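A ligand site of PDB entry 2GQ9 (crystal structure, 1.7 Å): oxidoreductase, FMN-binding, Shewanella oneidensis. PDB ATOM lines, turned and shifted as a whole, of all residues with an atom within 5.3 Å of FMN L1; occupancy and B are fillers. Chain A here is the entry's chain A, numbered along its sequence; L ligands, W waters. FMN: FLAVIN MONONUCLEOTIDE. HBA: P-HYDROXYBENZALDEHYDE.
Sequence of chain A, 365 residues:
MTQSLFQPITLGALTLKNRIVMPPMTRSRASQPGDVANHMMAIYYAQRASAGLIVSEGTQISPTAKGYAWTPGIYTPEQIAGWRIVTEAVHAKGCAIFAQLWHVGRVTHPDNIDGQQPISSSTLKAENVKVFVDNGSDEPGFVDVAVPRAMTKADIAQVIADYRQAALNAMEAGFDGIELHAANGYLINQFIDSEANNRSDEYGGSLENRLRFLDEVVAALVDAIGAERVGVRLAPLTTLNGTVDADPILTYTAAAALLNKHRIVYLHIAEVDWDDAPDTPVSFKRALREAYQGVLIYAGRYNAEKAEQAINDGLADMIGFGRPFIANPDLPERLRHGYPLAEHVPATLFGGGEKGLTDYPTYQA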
ATOM      1  N   PRO A  23       5.035 -14.003  -0.927  1.00  0.00           N
ATOM      2  CA  PRO A  23       6.102 -14.704  -1.653  1.00  0.00           C
ATOM      3  C   PRO A  23       7.364 -14.827  -0.844  1.00  0.00           C
ATOM      4  O   PRO A  23       7.566 -14.106   0.126  1.00  0.00           O
ATOM      5  CB  PRO A  23       6.287 -13.839  -2.907  1.00  0.00           C
ATOM      6  CG  PRO A  23       6.079 -12.467  -2.359  1.00  0.00           C
ATOM      7  CD  PRO A  23       4.878 -12.619  -1.425  1.00  0.00           C
ATOM      8  N   PRO A  24       8.236 -15.766  -1.231  1.00  0.00           N
ATOM      9  CA  PRO A  24       9.499 -15.980  -0.510  1.00  0.00           C
ATOM     10  C   PRO A  24      10.349 -14.724  -0.516  1.00  0.00           C
ATOM     11  O   PRO A  24      10.611 -14.171  -1.580  1.00  0.00           O
ATOM     12  CB  PRO A  24      10.155 -17.129  -1.287  1.00  0.00           C
ATOM     13  CG  PRO A  24       9.606 -16.961  -2.673  1.00  0.00           C
ATOM     14  CD  PRO A  24       8.158 -16.635  -2.421  1.00  0.00           C
ATOM     15  N   MET A  25      10.775 -14.287   0.667  1.00  0.00           N
ATOM     16  CA  MET A  25      11.613 -13.095   0.750  1.00  0.00           C
ATOM     17  C   MET A  25      12.722 -13.189   1.783  1.00  0.00           C
ATOM     18  O   MET A  25      12.497 -13.153   2.996  1.00  0.00           O
ATOM     19  CB  MET A  25      10.781 -11.833   0.998  1.00  0.00           C
ATOM     20  CG  MET A  25       9.916 -11.451  -0.193  1.00  0.00           C
ATOM     21  SD  MET A  25       8.961  -9.967   0.087  1.00  0.00           S
ATOM     22  CE  MET A  25       7.830 -10.519   1.382  1.00  0.00           C
ATOM     23  N   THR A  26      13.935 -13.339   1.273  1.00  0.00           N
ATOM     24  CA  THR A  26      15.154 -13.418   2.070  1.00  0.00           C
ATOM     25  C   THR A  26      15.297 -12.136   2.874  1.00  0.00           C
ATOM     26  O   THR A  26      15.265 -11.047   2.316  1.00  0.00           O
ATOM     27  CB  THR A  26      16.373 -13.558   1.145  1.00  0.00           C
ATOM     28  OG1 THR A  26      16.302 -14.829   0.478  1.00  0.00           O
ATOM     29  CG2 THR A  26      17.667 -13.451   1.926  1.00  0.00           C
ATOM     30  N   ARG A  27      15.438 -12.270   4.198  1.00  0.00           N
ATOM     31  CA  ARG A  27      15.607 -11.113   5.083  1.00  0.00           C
ATOM     32  C   ARG A  27      16.940 -11.230   5.823  1.00  0.00           C
ATOM     33  O   ARG A  27      17.350 -10.297   6.512  1.00  0.00           O
ATOM     34  CB  ARG A  27      14.448 -11.028   6.089  1.00  0.00           C
ATOM     35  CG  ARG A  27      13.056 -10.943   5.469  1.00  0.00           C
ATOM     36  CD  ARG A  27      12.963  -9.845   4.410  1.00  0.00           C
ATOM     37  NE  ARG A  27      13.267  -8.530   4.975  1.00  0.00           N
ATOM     38  CZ  ARG A  27      12.430  -7.792   5.703  1.00  0.00           C
ATOM     39  NH1 ARG A  27      11.191  -8.216   5.956  1.00  0.00           N
ATOM     40  NH2 ARG A  27      12.841  -6.637   6.186  1.00  0.00           N
ATOM     41  N   GLU A  57      11.130 -17.477   3.170  1.00  0.00           N
ATOM     42  CA  GLU A  57      12.316 -16.984   2.483  1.00  0.00           C
ATOM     43  C   GLU A  57      13.098 -18.237   2.092  1.00  0.00           C
ATOM     44  O   GLU A  57      12.950 -19.291   2.705  1.00  0.00           O
ATOM     45  CB  GLU A  57      13.171 -16.186   3.468  1.00  0.00           C
ATOM     46  CG  GLU A  57      13.533 -17.005   4.704  1.00  0.00           C
ATOM     47  CD  GLU A  57      13.756 -16.155   5.952  1.00  0.00           C
ATOM     48  OE1 GLU A  57      14.919 -15.794   6.227  1.00  0.00           O
ATOM     49  OE2 GLU A  57      12.769 -15.844   6.644  1.00  0.00           O
ATOM     50  N   GLY A  58      13.937 -18.127   1.067  1.00  0.00           N
ATOM     51  CA  GLY A  58      14.735 -19.275   0.678  1.00  0.00           C
ATOM     52  C   GLY A  58      15.515 -19.809   1.866  1.00  0.00           C
ATOM     53  O   GLY A  58      16.059 -19.047   2.674  1.00  0.00           O
ATOM     54  N   GLN A 100      10.601 -22.630   1.226  1.00  0.00           N
ATOM     55  CA  GLN A 100      11.223 -22.575  -0.093  1.00  0.00           C
ATOM     56  C   GLN A 100      12.608 -23.196  -0.015  1.00  0.00           C
ATOM     57  O   GLN A 100      13.538 -22.606   0.546  1.00  0.00           O
ATOM     58  CB  GLN A 100      11.351 -21.139  -0.635  1.00  0.00           C
ATOM     59  CG  GLN A 100      11.903 -21.151  -2.067  1.00  0.00           C
ATOM     60  CD  GLN A 100      12.213 -19.783  -2.622  1.00  0.00           C
ATOM     61  OE1 GLN A 100      13.032 -19.059  -2.079  1.00  0.00           O
ATOM     62  NE2 GLN A 100      11.577 -19.445  -3.735  1.00  0.00           N
ATOM     63  N   TRP A 102      16.095 -24.062  -1.043  1.00  0.00           N
ATOM     64  CA  TRP A 102      17.053 -23.307  -1.839  1.00  0.00           C
ATOM     65  C   TRP A 102      18.440 -23.889  -2.053  1.00  0.00           C
ATOM     66  O   TRP A 102      19.046 -24.458  -1.139  1.00  0.00           O
ATOM     67  CB  TRP A 102      17.202 -21.961  -1.143  1.00  0.00           C
ATOM     68  CG  TRP A 102      17.717 -20.803  -1.926  1.00  0.00           C
ATOM     69  CD1 TRP A 102      17.801 -20.670  -3.286  1.00  0.00           C
ATOM     70  CD2 TRP A 102      18.095 -19.529  -1.378  1.00  0.00           C
ATOM     71  NE1 TRP A 102      18.190 -19.392  -3.620  1.00  0.00           N
ATOM     72  CE2 TRP A 102      18.381 -18.674  -2.461  1.00  0.00           C
ATOM     73  CE3 TRP A 102      18.219 -19.038  -0.069  1.00  0.00           C
ATOM     74  CZ2 TRP A 102      18.765 -17.344  -2.279  1.00  0.00           C
ATOM     75  CZ3 TRP A 102      18.603 -17.722   0.114  1.00  0.00           C
ATOM     76  CH2 TRP A 102      18.876 -16.889  -0.985  1.00  0.00           C
ATOM     77  N   GLU A 179       8.397 -25.352  -1.424  1.00  0.00           N
ATOM     78  CA  GLU A 179       8.425 -24.716  -2.741  1.00  0.00           C
ATOM     79  C   GLU A 179       9.836 -24.893  -3.269  1.00  0.00           C
ATOM     80  O   GLU A 179      10.810 -24.478  -2.628  1.00  0.00           O
ATOM     81  CB  GLU A 179       8.111 -23.219  -2.677  1.00  0.00           C
ATOM     82  CG  GLU A 179       8.104 -22.586  -4.078  1.00  0.00           C
ATOM     83  CD  GLU A 179       7.814 -21.100  -4.062  1.00  0.00           C
ATOM     84  OE1 GLU A 179       8.780 -20.303  -4.056  1.00  0.00           O
ATOM     85  OE2 GLU A 179       6.618 -20.731  -4.041  1.00  0.00           O
ATOM     86  N   HIS A 181      12.800 -23.828  -5.243  1.00  0.00           N
ATOM     87  CA  HIS A 181      13.261 -22.586  -5.862  1.00  0.00           C
ATOM     88  C   HIS A 181      14.017 -22.954  -7.133  1.00  0.00           C
ATOM     89  O   HIS A 181      15.197 -23.310  -7.078  1.00  0.00           O
ATOM     90  CB  HIS A 181      14.195 -21.803  -4.937  1.00  0.00           C
ATOM     91  CG  HIS A 181      14.407 -20.380  -5.377  1.00  0.00           C
ATOM     92  ND1 HIS A 181      14.051 -19.925  -6.629  1.00  0.00           N
ATOM     93  CD2 HIS A 181      14.900 -19.305  -4.715  1.00  0.00           C
ATOM     94  CE1 HIS A 181      14.311 -18.640  -6.723  1.00  0.00           C
ATOM     95  NE2 HIS A 181      14.829 -18.224  -5.572  1.00  0.00           N
ATOM     96  N   ASN A 184      14.993 -17.355 -10.417  1.00  0.00           N
ATOM     97  CA  ASN A 184      15.937 -16.282 -10.201  1.00  0.00           C
ATOM     98  C   ASN A 184      17.416 -16.574 -10.338  1.00  0.00           C
ATOM     99  O   ASN A 184      18.245 -16.051  -9.582  1.00  0.00           O
ATOM    100  CB  ASN A 184      15.599 -15.607  -8.864  1.00  0.00           C
ATOM    101  CG  ASN A 184      14.146 -15.173  -8.812  1.00  0.00           C
ATOM    102  OD1 ASN A 184      13.497 -15.070  -9.849  1.00  0.00           O
ATOM    103  ND2 ASN A 184      13.635 -14.915  -7.608  1.00  0.00           N
ATOM    104  N   ARG A 233       8.864 -22.937  -8.121  1.00  0.00           N
ATOM    105  CA  ARG A 233       8.900 -21.564  -8.606  1.00  0.00           C
ATOM    106  C   ARG A 233       9.836 -21.434  -9.801  1.00  0.00           C
ATOM    107  O   ARG A 233      10.961 -21.937  -9.777  1.00  0.00           O
ATOM    108  CB  ARG A 233       9.359 -20.608  -7.496  1.00  0.00           C
ATOM    109  CG  ARG A 233       8.981 -19.165  -7.816  1.00  0.00           C
ATOM    110  CD  ARG A 233       9.374 -18.152  -6.754  1.00  0.00           C
ATOM    111  NE  ARG A 233       8.435 -17.022  -6.803  1.00  0.00           N
ATOM    112  CZ  ARG A 233       8.682 -15.783  -6.385  1.00  0.00           C
ATOM    113  NH1 ARG A 233       9.848 -15.478  -5.850  1.00  0.00           N
ATOM    114  NH2 ARG A 233       7.742 -14.861  -6.466  1.00  0.00           N
ATOM    115  N   ALA A 270       7.685 -16.131 -10.991  1.00  0.00           N
ATOM    116  CA  ALA A 270       8.295 -14.896 -10.522  1.00  0.00           C
ATOM    117  C   ALA A 270       8.389 -14.019 -11.763  1.00  0.00           C
ATOM    118  O   ALA A 270       9.266 -14.212 -12.609  1.00  0.00           O
ATOM    119  CB  ALA A 270       9.684 -15.162  -9.955  1.00  0.00           C
ATOM    120  N   VAL A 272       8.684 -10.582 -11.789  1.00  0.00           N
ATOM    121  CA  VAL A 272       9.576  -9.452 -11.624  1.00  0.00           C
ATOM    122  C   VAL A 272      10.578  -9.778 -10.543  1.00  0.00           C
ATOM    123  O   VAL A 272      10.260 -10.445  -9.553  1.00  0.00           O
ATOM    124  CB  VAL A 272       8.785  -8.183 -11.211  1.00  0.00           C
ATOM    125  CG1 VAL A 272       9.747  -7.029 -10.920  1.00  0.00           C
ATOM    126  CG2 VAL A 272       7.811  -7.803 -12.312  1.00  0.00           C
ATOM    127  N   ASP A 273      11.816  -9.337 -10.745  1.00  0.00           N
ATOM    128  CA  ASP A 273      12.874  -9.544  -9.766  1.00  0.00           C
ATOM    129  C   ASP A 273      13.500  -8.160  -9.627  1.00  0.00           C
ATOM    130  O   ASP A 273      14.272  -7.738 -10.485  1.00  0.00           O
ATOM    131  CB  ASP A 273      13.884 -10.570 -10.277  1.00  0.00           C
ATOM    132  CG  ASP A 273      14.692 -11.202  -9.153  1.00  0.00           C
ATOM    133  OD1 ASP A 273      14.103 -11.465  -8.081  1.00  0.00           O
ATOM    134  OD2 ASP A 273      15.897 -11.453  -9.346  1.00  0.00           O
ATOM    135  N   TRP A 274      13.143  -7.471  -8.545  1.00  0.00           N
ATOM    136  CA  TRP A 274      13.626  -6.122  -8.296  1.00  0.00           C
ATOM    137  C   TRP A 274      13.077  -5.197  -9.376  1.00  0.00           C
ATOM    138  O   TRP A 274      11.864  -5.043  -9.506  1.00  0.00           O
ATOM    139  CB  TRP A 274      15.151  -6.100  -8.253  1.00  0.00           C
ATOM    140  CG  TRP A 274      15.689  -6.886  -7.115  1.00  0.00           C
ATOM    141  CD1 TRP A 274      16.349  -8.076  -7.167  1.00  0.00           C
ATOM    142  CD2 TRP A 274      15.536  -6.566  -5.726  1.00  0.00           C
ATOM    143  NE1 TRP A 274      16.623  -8.526  -5.894  1.00  0.00           N
ATOM    144  CE2 TRP A 274      16.136  -7.613  -4.985  1.00  0.00           C
ATOM    145  CE3 TRP A 274      14.956  -5.497  -5.028  1.00  0.00           C
ATOM    146  CZ2 TRP A 274      16.173  -7.624  -3.589  1.00  0.00           C
ATOM    147  CZ3 TRP A 274      14.993  -5.508  -3.632  1.00  0.00           C
ATOM    148  CH2 TRP A 274      15.597  -6.572  -2.932  1.00  0.00           C
ATOM    149  N   ALA A 299       3.752 -13.463  -9.095  1.00  0.00           N
ATOM    150  CA  ALA A 299       4.191 -12.392  -8.213  1.00  0.00           C
ATOM    151  C   ALA A 299       5.080 -11.442  -9.020  1.00  0.00           C
ATOM    152  O   ALA A 299       5.824 -11.886  -9.913  1.00  0.00           O
ATOM    153  CB  ALA A 299       4.981 -12.942  -7.036  1.00  0.00           C
ATOM    154  N   GLY A 300       4.991 -10.163  -8.725  1.00  0.00           N
ATOM    155  CA  GLY A 300       5.812  -9.182  -9.435  1.00  0.00           C
ATOM    156  C   GLY A 300       5.057  -7.933  -9.805  1.00  0.00           C
ATOM    157  O   GLY A 300       4.307  -7.913 -10.781  1.00  0.00           O
ATOM    158  N   ARG A 301       5.241  -6.881  -9.001  1.00  0.00           N
ATOM    159  CA  ARG A 301       4.608  -5.594  -9.218  1.00  0.00           C
ATOM    160  C   ARG A 301       3.093  -5.575  -9.286  1.00  0.00           C
ATOM    161  O   ARG A 301       2.510  -4.723  -9.961  1.00  0.00           O
ATOM    162  CB  ARG A 301       5.169  -4.937 -10.486  1.00  0.00           C
ATOM    163  CG  ARG A 301       6.648  -4.577 -10.405  1.00  0.00           C
ATOM    164  CD  ARG A 301       6.913  -3.622  -9.256  1.00  0.00           C
ATOM    165  NE  ARG A 301       8.275  -3.078  -9.288  1.00  0.00           N
ATOM    166  CZ  ARG A 301       8.870  -2.482  -8.259  1.00  0.00           C
ATOM    167  NH1 ARG A 301       8.227  -2.355  -7.108  1.00  0.00           N
ATOM    168  NH2 ARG A 301      10.109  -2.015  -8.380  1.00  0.00           N
ATOM    169  N   TYR A 302       2.431  -6.510  -8.599  1.00  0.00           N
ATOM    170  CA  TYR A 302       0.974  -6.505  -8.609  1.00  0.00           C
ATOM    171  C   TYR A 302       0.407  -5.551  -7.567  1.00  0.00           C
ATOM    172  O   TYR A 302       1.011  -5.323  -6.513  1.00  0.00           O
ATOM    173  CB  TYR A 302       0.441  -7.911  -8.316  1.00  0.00           C
ATOM    174  CG  TYR A 302       0.462  -8.842  -9.498  1.00  0.00           C
ATOM    175  CD1 TYR A 302      -0.631  -8.923 -10.362  1.00  0.00           C
ATOM    176  CD2 TYR A 302       1.585  -9.612  -9.781  1.00  0.00           C
ATOM    177  CE1 TYR A 302      -0.600  -9.738 -11.479  1.00  0.00           C
ATOM    178  CE2 TYR A 302       1.638 -10.421 -10.904  1.00  0.00           C
ATOM    179  CZ  TYR A 302       0.541 -10.480 -11.758  1.00  0.00           C
ATOM    180  OH  TYR A 302       0.596 -11.246 -12.884  1.00  0.00           O
ATOM    181  N   GLY A 320       1.026 -13.178  -5.550  1.00  0.00           N
ATOM    182  CA  GLY A 320       1.937 -12.825  -4.476  1.00  0.00           C
ATOM    183  C   GLY A 320       2.253 -11.333  -4.491  1.00  0.00           C
ATOM    184  O   GLY A 320       2.331 -10.713  -5.551  1.00  0.00           O
ATOM    185  N   PHE A 321       2.404 -10.759  -3.305  1.00  0.00           N
ATOM    186  CA  PHE A 321       2.733  -9.341  -3.134  1.00  0.00           C
ATOM    187  C   PHE A 321       3.953  -9.399  -2.224  1.00  0.00           C
ATOM    188  O   PHE A 321       3.826  -9.762  -1.059  1.00  0.00           O
ATOM    189  CB  PHE A 321       1.615  -8.575  -2.428  1.00  0.00           C
ATOM    190  CG  PHE A 321       0.315  -8.545  -3.182  1.00  0.00           C
ATOM    191  CD1 PHE A 321       0.009  -7.471  -4.010  1.00  0.00           C
ATOM    192  CD2 PHE A 321      -0.591  -9.601  -3.078  1.00  0.00           C
ATOM    193  CE1 PHE A 321      -1.180  -7.446  -4.730  1.00  0.00           C
ATOM    194  CE2 PHE A 321      -1.787  -9.582  -3.796  1.00  0.00           C
ATOM    195  CZ  PHE A 321      -2.085  -8.501  -4.626  1.00  0.00           C
ATOM    196  N   GLY A 322       5.127  -9.037  -2.747  1.00  0.00           N
ATOM    197  CA  GLY A 322       6.325  -9.122  -1.944  1.00  0.00           C
ATOM    198  C   GLY A 322       6.689  -7.902  -1.142  1.00  0.00           C
ATOM    199  O   GLY A 322       6.502  -7.847   0.071  1.00  0.00           O
ATOM    200  N   ARG A 323       7.231  -6.897  -1.832  1.00  0.00           N
ATOM    201  CA  ARG A 323       7.626  -5.671  -1.142  1.00  0.00           C
ATOM    202  C   ARG A 323       6.515  -5.053  -0.307  1.00  0.00           C
ATOM    203  O   ARG A 323       6.757  -4.630   0.820  1.00  0.00           O
ATOM    204  CB  ARG A 323       8.221  -4.696  -2.165  1.00  0.00           C
ATOM    205  CG  ARG A 323       9.640  -5.170  -2.547  1.00  0.00           C
ATOM    206  CD  ARG A 323      10.197  -4.555  -3.823  1.00  0.00           C
ATOM    207  NE  ARG A 323       9.706  -5.230  -5.020  1.00  0.00           N
ATOM    208  CZ  ARG A 323      10.174  -5.005  -6.245  1.00  0.00           C
ATOM    209  NH1 ARG A 323       9.674  -5.663  -7.286  1.00  0.00           N
ATOM    210  NH2 ARG A 323      11.152  -4.114  -6.422  1.00  0.00           N
ATOM    211  N   PRO A 324       5.276  -5.027  -0.819  1.00  0.00           N
ATOM    212  CA  PRO A 324       4.213  -4.442  -0.016  1.00  0.00           C
ATOM    213  C   PRO A 324       3.991  -5.238   1.276  1.00  0.00           C
ATOM    214  O   PRO A 324       3.576  -4.665   2.275  1.00  0.00           O
ATOM    215  CB  PRO A 324       3.006  -4.514  -0.954  1.00  0.00           C
ATOM    216  CG  PRO A 324       3.629  -4.384  -2.318  1.00  0.00           C
ATOM    217  CD  PRO A 324       4.806  -5.310  -2.194  1.00  0.00           C
ATOM    218  N   ILE A 326       6.297  -6.621   3.022  1.00  0.00           N
ATOM    219  CA  ILE A 326       7.374  -6.301   3.952  1.00  0.00           C
ATOM    220  C   ILE A 326       6.948  -5.136   4.855  1.00  0.00           C
ATOM    221  O   ILE A 326       7.062  -5.211   6.079  1.00  0.00           O
ATOM    222  CB  ILE A 326       8.688  -5.911   3.195  1.00  0.00           C
ATOM    223  CG1 ILE A 326       9.242  -7.143   2.469  1.00  0.00           C
ATOM    224  CG2 ILE A 326       9.727  -5.301   4.183  1.00  0.00           C
ATOM    225  CD1 ILE A 326      10.526  -6.909   1.696  1.00  0.00           C
ATOM    226  N   LEU A 349      16.211  -4.250   4.627  1.00  0.00           N
ATOM    227  CA  LEU A 349      15.706  -5.472   3.995  1.00  0.00           C
ATOM    228  C   LEU A 349      16.483  -6.694   4.472  1.00  0.00           C
ATOM    229  O   LEU A 349      15.906  -7.751   4.750  1.00  0.00           O
ATOM    230  CB  LEU A 349      15.819  -5.379   2.474  1.00  0.00           C
ATOM    231  CG  LEU A 349      14.763  -4.538   1.755  1.00  0.00           C
ATOM    232  CD1 LEU A 349      15.051  -4.502   0.275  1.00  0.00           C
ATOM    233  CD2 LEU A 349      13.358  -5.130   2.007  1.00  0.00           C
ATOM    234  N   PHE A 350      17.802  -6.544   4.583  1.00  0.00           N
ATOM    235  CA  PHE A 350      18.663  -7.641   4.981  1.00  0.00           C
ATOM    236  C   PHE A 350      19.518  -7.375   6.207  1.00  0.00           C
ATOM    237  O   PHE A 350      20.041  -6.272   6.395  1.00  0.00           O
ATOM    238  CB  PHE A 350      19.597  -8.026   3.840  1.00  0.00           C
ATOM    239  CG  PHE A 350      18.926  -8.117   2.508  1.00  0.00           C
ATOM    240  CD1 PHE A 350      19.019  -7.071   1.589  1.00  0.00           C
ATOM    241  CD2 PHE A 350      18.226  -9.262   2.150  1.00  0.00           C
ATOM    242  CE1 PHE A 350      18.424  -7.162   0.330  1.00  0.00           C
ATOM    243  CE2 PHE A 350      17.630  -9.367   0.891  1.00  0.00           C
ATOM    244  CZ  PHE A 350      17.725  -8.321  -0.017  1.00  0.00           C
HETATM  245  N1  FMN L   1      12.228 -14.705  -4.407  1.00  0.00           N
HETATM  246  C2  FMN L   1      12.522 -16.061  -4.152  1.00  0.00           C
HETATM  247  O2  FMN L   1      12.175 -16.931  -4.901  1.00  0.00           O
HETATM  248  N3  FMN L   1      13.205 -16.381  -2.917  1.00  0.00           N
HETATM  249  C4  FMN L   1      13.619 -15.489  -1.968  1.00  0.00           C
HETATM  250  O4  FMN L   1      14.282 -15.845  -1.006  1.00  0.00           O
HETATM  251  C4A FMN L   1      13.428 -14.049  -2.274  1.00  0.00           C
HETATM  252  N5  FMN L   1      14.077 -13.077  -1.544  1.00  0.00           N
HETATM  253  C5A FMN L   1      13.663 -11.781  -1.735  1.00  0.00           C
HETATM  254  C6  FMN L   1      14.118 -10.735  -0.783  1.00  0.00           C
HETATM  255  C7  FMN L   1      13.617  -9.376  -0.841  1.00  0.00           C
HETATM  256  C7M FMN L   1      14.048  -8.385   0.233  1.00  0.00           C
HETATM  257  C8  FMN L   1      12.705  -9.012  -1.926  1.00  0.00           C
HETATM  258  C8M FMN L   1      12.076  -7.598  -2.016  1.00  0.00           C
HETATM  259  C9  FMN L   1      12.296 -10.019  -2.881  1.00  0.00           C
HETATM  260  C9A FMN L   1      12.756 -11.361  -2.814  1.00  0.00           C
HETATM  261  N10 FMN L   1      12.306 -12.458  -3.672  1.00  0.00           N
HETATM  262  C10 FMN L   1      12.658 -13.783  -3.546  1.00  0.00           C
HETATM  263  C1' FMN L   1      11.411 -12.093  -4.833  1.00  0.00           C
HETATM  264  C2' FMN L   1       9.966 -12.017  -4.354  1.00  0.00           C
HETATM  265  O2' FMN L   1       9.453 -13.273  -3.907  1.00  0.00           O
HETATM  266  C3' FMN L   1       9.003 -11.450  -5.405  1.00  0.00           C
HETATM  267  O3' FMN L   1       8.884 -12.368  -6.510  1.00  0.00           O
HETATM  268  C4' FMN L   1       9.458 -10.096  -5.934  1.00  0.00           C
HETATM  269  O4' FMN L   1       9.757  -9.168  -4.844  1.00  0.00           O
HETATM  270  C5' FMN L   1       8.474  -9.458  -6.889  1.00  0.00           C
HETATM  271  O5' FMN L   1       7.218  -9.110  -6.202  1.00  0.00           O
HETATM  272  P   FMN L   1       6.870  -7.654  -5.683  1.00  0.00           P
HETATM  273  O1P FMN L   1       7.775  -7.290  -4.547  1.00  0.00           O
HETATM  274  O2P FMN L   1       6.966  -6.717  -6.877  1.00  0.00           O
HETATM  275  O3P FMN L   1       5.407  -7.767  -5.190  1.00  0.00           O
HETATM  276  C1' HBA L   2      17.605 -11.591  -2.245  1.00  0.00           C
HETATM  277  O1' HBA L   2      17.480 -10.408  -2.504  1.00  0.00           O
HETATM  278  C1  HBA L   2      16.988 -12.608  -3.095  1.00  0.00           C
HETATM  279  C2  HBA L   2      17.135 -13.995  -2.780  1.00  0.00           C
HETATM  280  C3  HBA L   2      16.596 -14.953  -3.652  1.00  0.00           C
HETATM  281  C4  HBA L   2      15.915 -14.537  -4.820  1.00  0.00           C
HETATM  282  C5  HBA L   2      15.719 -13.177  -5.152  1.00  0.00           C
HETATM  283  C6  HBA L   2      16.251 -12.238  -4.266  1.00  0.00           C
HETATM  284  O4  HBA L   2      15.173 -15.470  -5.466  1.00  0.00           O
HETATM  285  O   HOH W   1       3.526  -5.727  -5.267  1.00  0.00           O
HETATM  286  O   HOH W   2      11.327 -12.378  -7.981  1.00  0.00           O
HETATM  287  O   HOH W   3      14.227  -9.745  -5.681  1.00  0.00           O
HETATM  288  O   HOH W   4       6.308  -3.916  -5.772  1.00  0.00           O
HETATM  289  O   HOH W   5       3.470  -8.699  -6.833  1.00  0.00           O
HETATM  290  O   HOH W   6      12.224  -8.221  -5.972  1.00  0.00           O
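N of Thr 26 is in hydrogen-bond range of N5 of FMN L1, 2.8 Å away. An oxygen (O4) of FMN L1 lies within hydrogen-bond range of the side-chain hydroxyl (OG1) of Thr 26, at 2.7 Å. The backbone NH of Arg 301 lies within hydrogen-bond range of an oxygen (O2P) of FMN L1, 2.7 Å away. NH2 of Arg 233 sits at hydrogen-bond distance from O3' of FMN L1, at 2.7 Å. The backbone carbonyl oxygen of Pro 24 sits at hydrogen-bond distance from an oxygen (O2') of FMN L1. O3P of FMN L1 lies within hydrogen-bond range of N of Gly 322 (2.8 Å). The backbone NH (N) of Arg 323 sits at hydrogen-bond distance from an oxygen (O1P) of FMN L1 (2.8 Å). O1P of FMN L1 is in salt-bridge range of NE of Arg 323 (2.9 Å). The side-chain amide oxygen of Gln 100 sits at hydrogen-bond distance from a nitrogen (N3) of FMN L1. A ring nitrogen (NE2) of His 181 sits at hydrogen-bond distance from an oxygen (O2) of FMN L1, at 3.0 Å. An oxygen (O4) of FMN L1 lies within hydrogen-bond range of the backbone NH (N) of Gly 58, 3.1 Å away. An oxygen (O4) of HBA L2 lies within hydrogen-bond range of a ring nitrogen (NE2) of His 181. The side-chain amide nitrogen of Asn 184 sits at hydrogen-bond distance from an oxygen (O4) of HBA L2 (2.7 Å).
N1 of FMN L1 sits close to O4 of HBA L2 (3.2 Å).
The guanidinium group (NH1) of Arg 323 lies within hydrogen-bond range of the backbone carbonyl oxygen (O) of Trp 274 (3.2 Å). OE1 of Gln 100 lies close to N of Gly 58. OE1 of Glu 179 is in hydrogen-bond range of NE2 of Gln 100. The guanidinium group of Arg 27 sits at hydrogen-bond distance from the backbone carbonyl oxygen of Leu 349.
Pro 23 touches FMN L1. Met 25 touches FMN L1 (CA to N5, 3.4 Å). Asn 184 touches FMN L1 (ND2 to N1, 3.5 Å). O of Val 272 touches C5' of FMN L1, at 3.4 Å. Trp 274 touches FMN L1. Ala 299 touches FMN L1 (CB to O3', 3.98 Å). N of Gly 300 touches O5' of FMN L1 (3.5 Å). Phe 321 touches FMN L1 (C to O3P, 3.7 Å). Pro 324 touches FMN L1 (CD to O3P, 3.9 Å). Leu 349 touches FMN L1 (CD2 to C7M, 3.8 Å). Phe 350 touches FMN L1. 20 residues have an atom within 4 Å of FMN L1: Pro 23, Pro 24, Met 25, Thr 26, Gly 58, Gln 100, His 181, Asn 184, Arg 233, Val 272, Trp 274, Ala 299, Gly 300, Arg 301, Phe 321, Gly 322, Arg 323, Pro 324, Leu 349 and Phe 350.
Water W1 bridges O3P of FMN L1 and O of Tyr 302. Water W2 lies within hydrogen-bond range of O of Val 272 (2.7 Å), O3' of FMN L1 (2.9 Å), OD1 of Asp 273 (2.9 Å) and ND2 of Asn 184 (3.4 Å). Water W6 bridges N of Trp 274 and O4' of FMN L1. Water W4 lies within hydrogen-bond range of NH1 of Arg 301 (2.8 Å) and O2P of FMN L1 (3.1 Å). Water W3 bridges the indole nitrogen of Trp 274 and the side-chain carboxylate of Asp 273.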
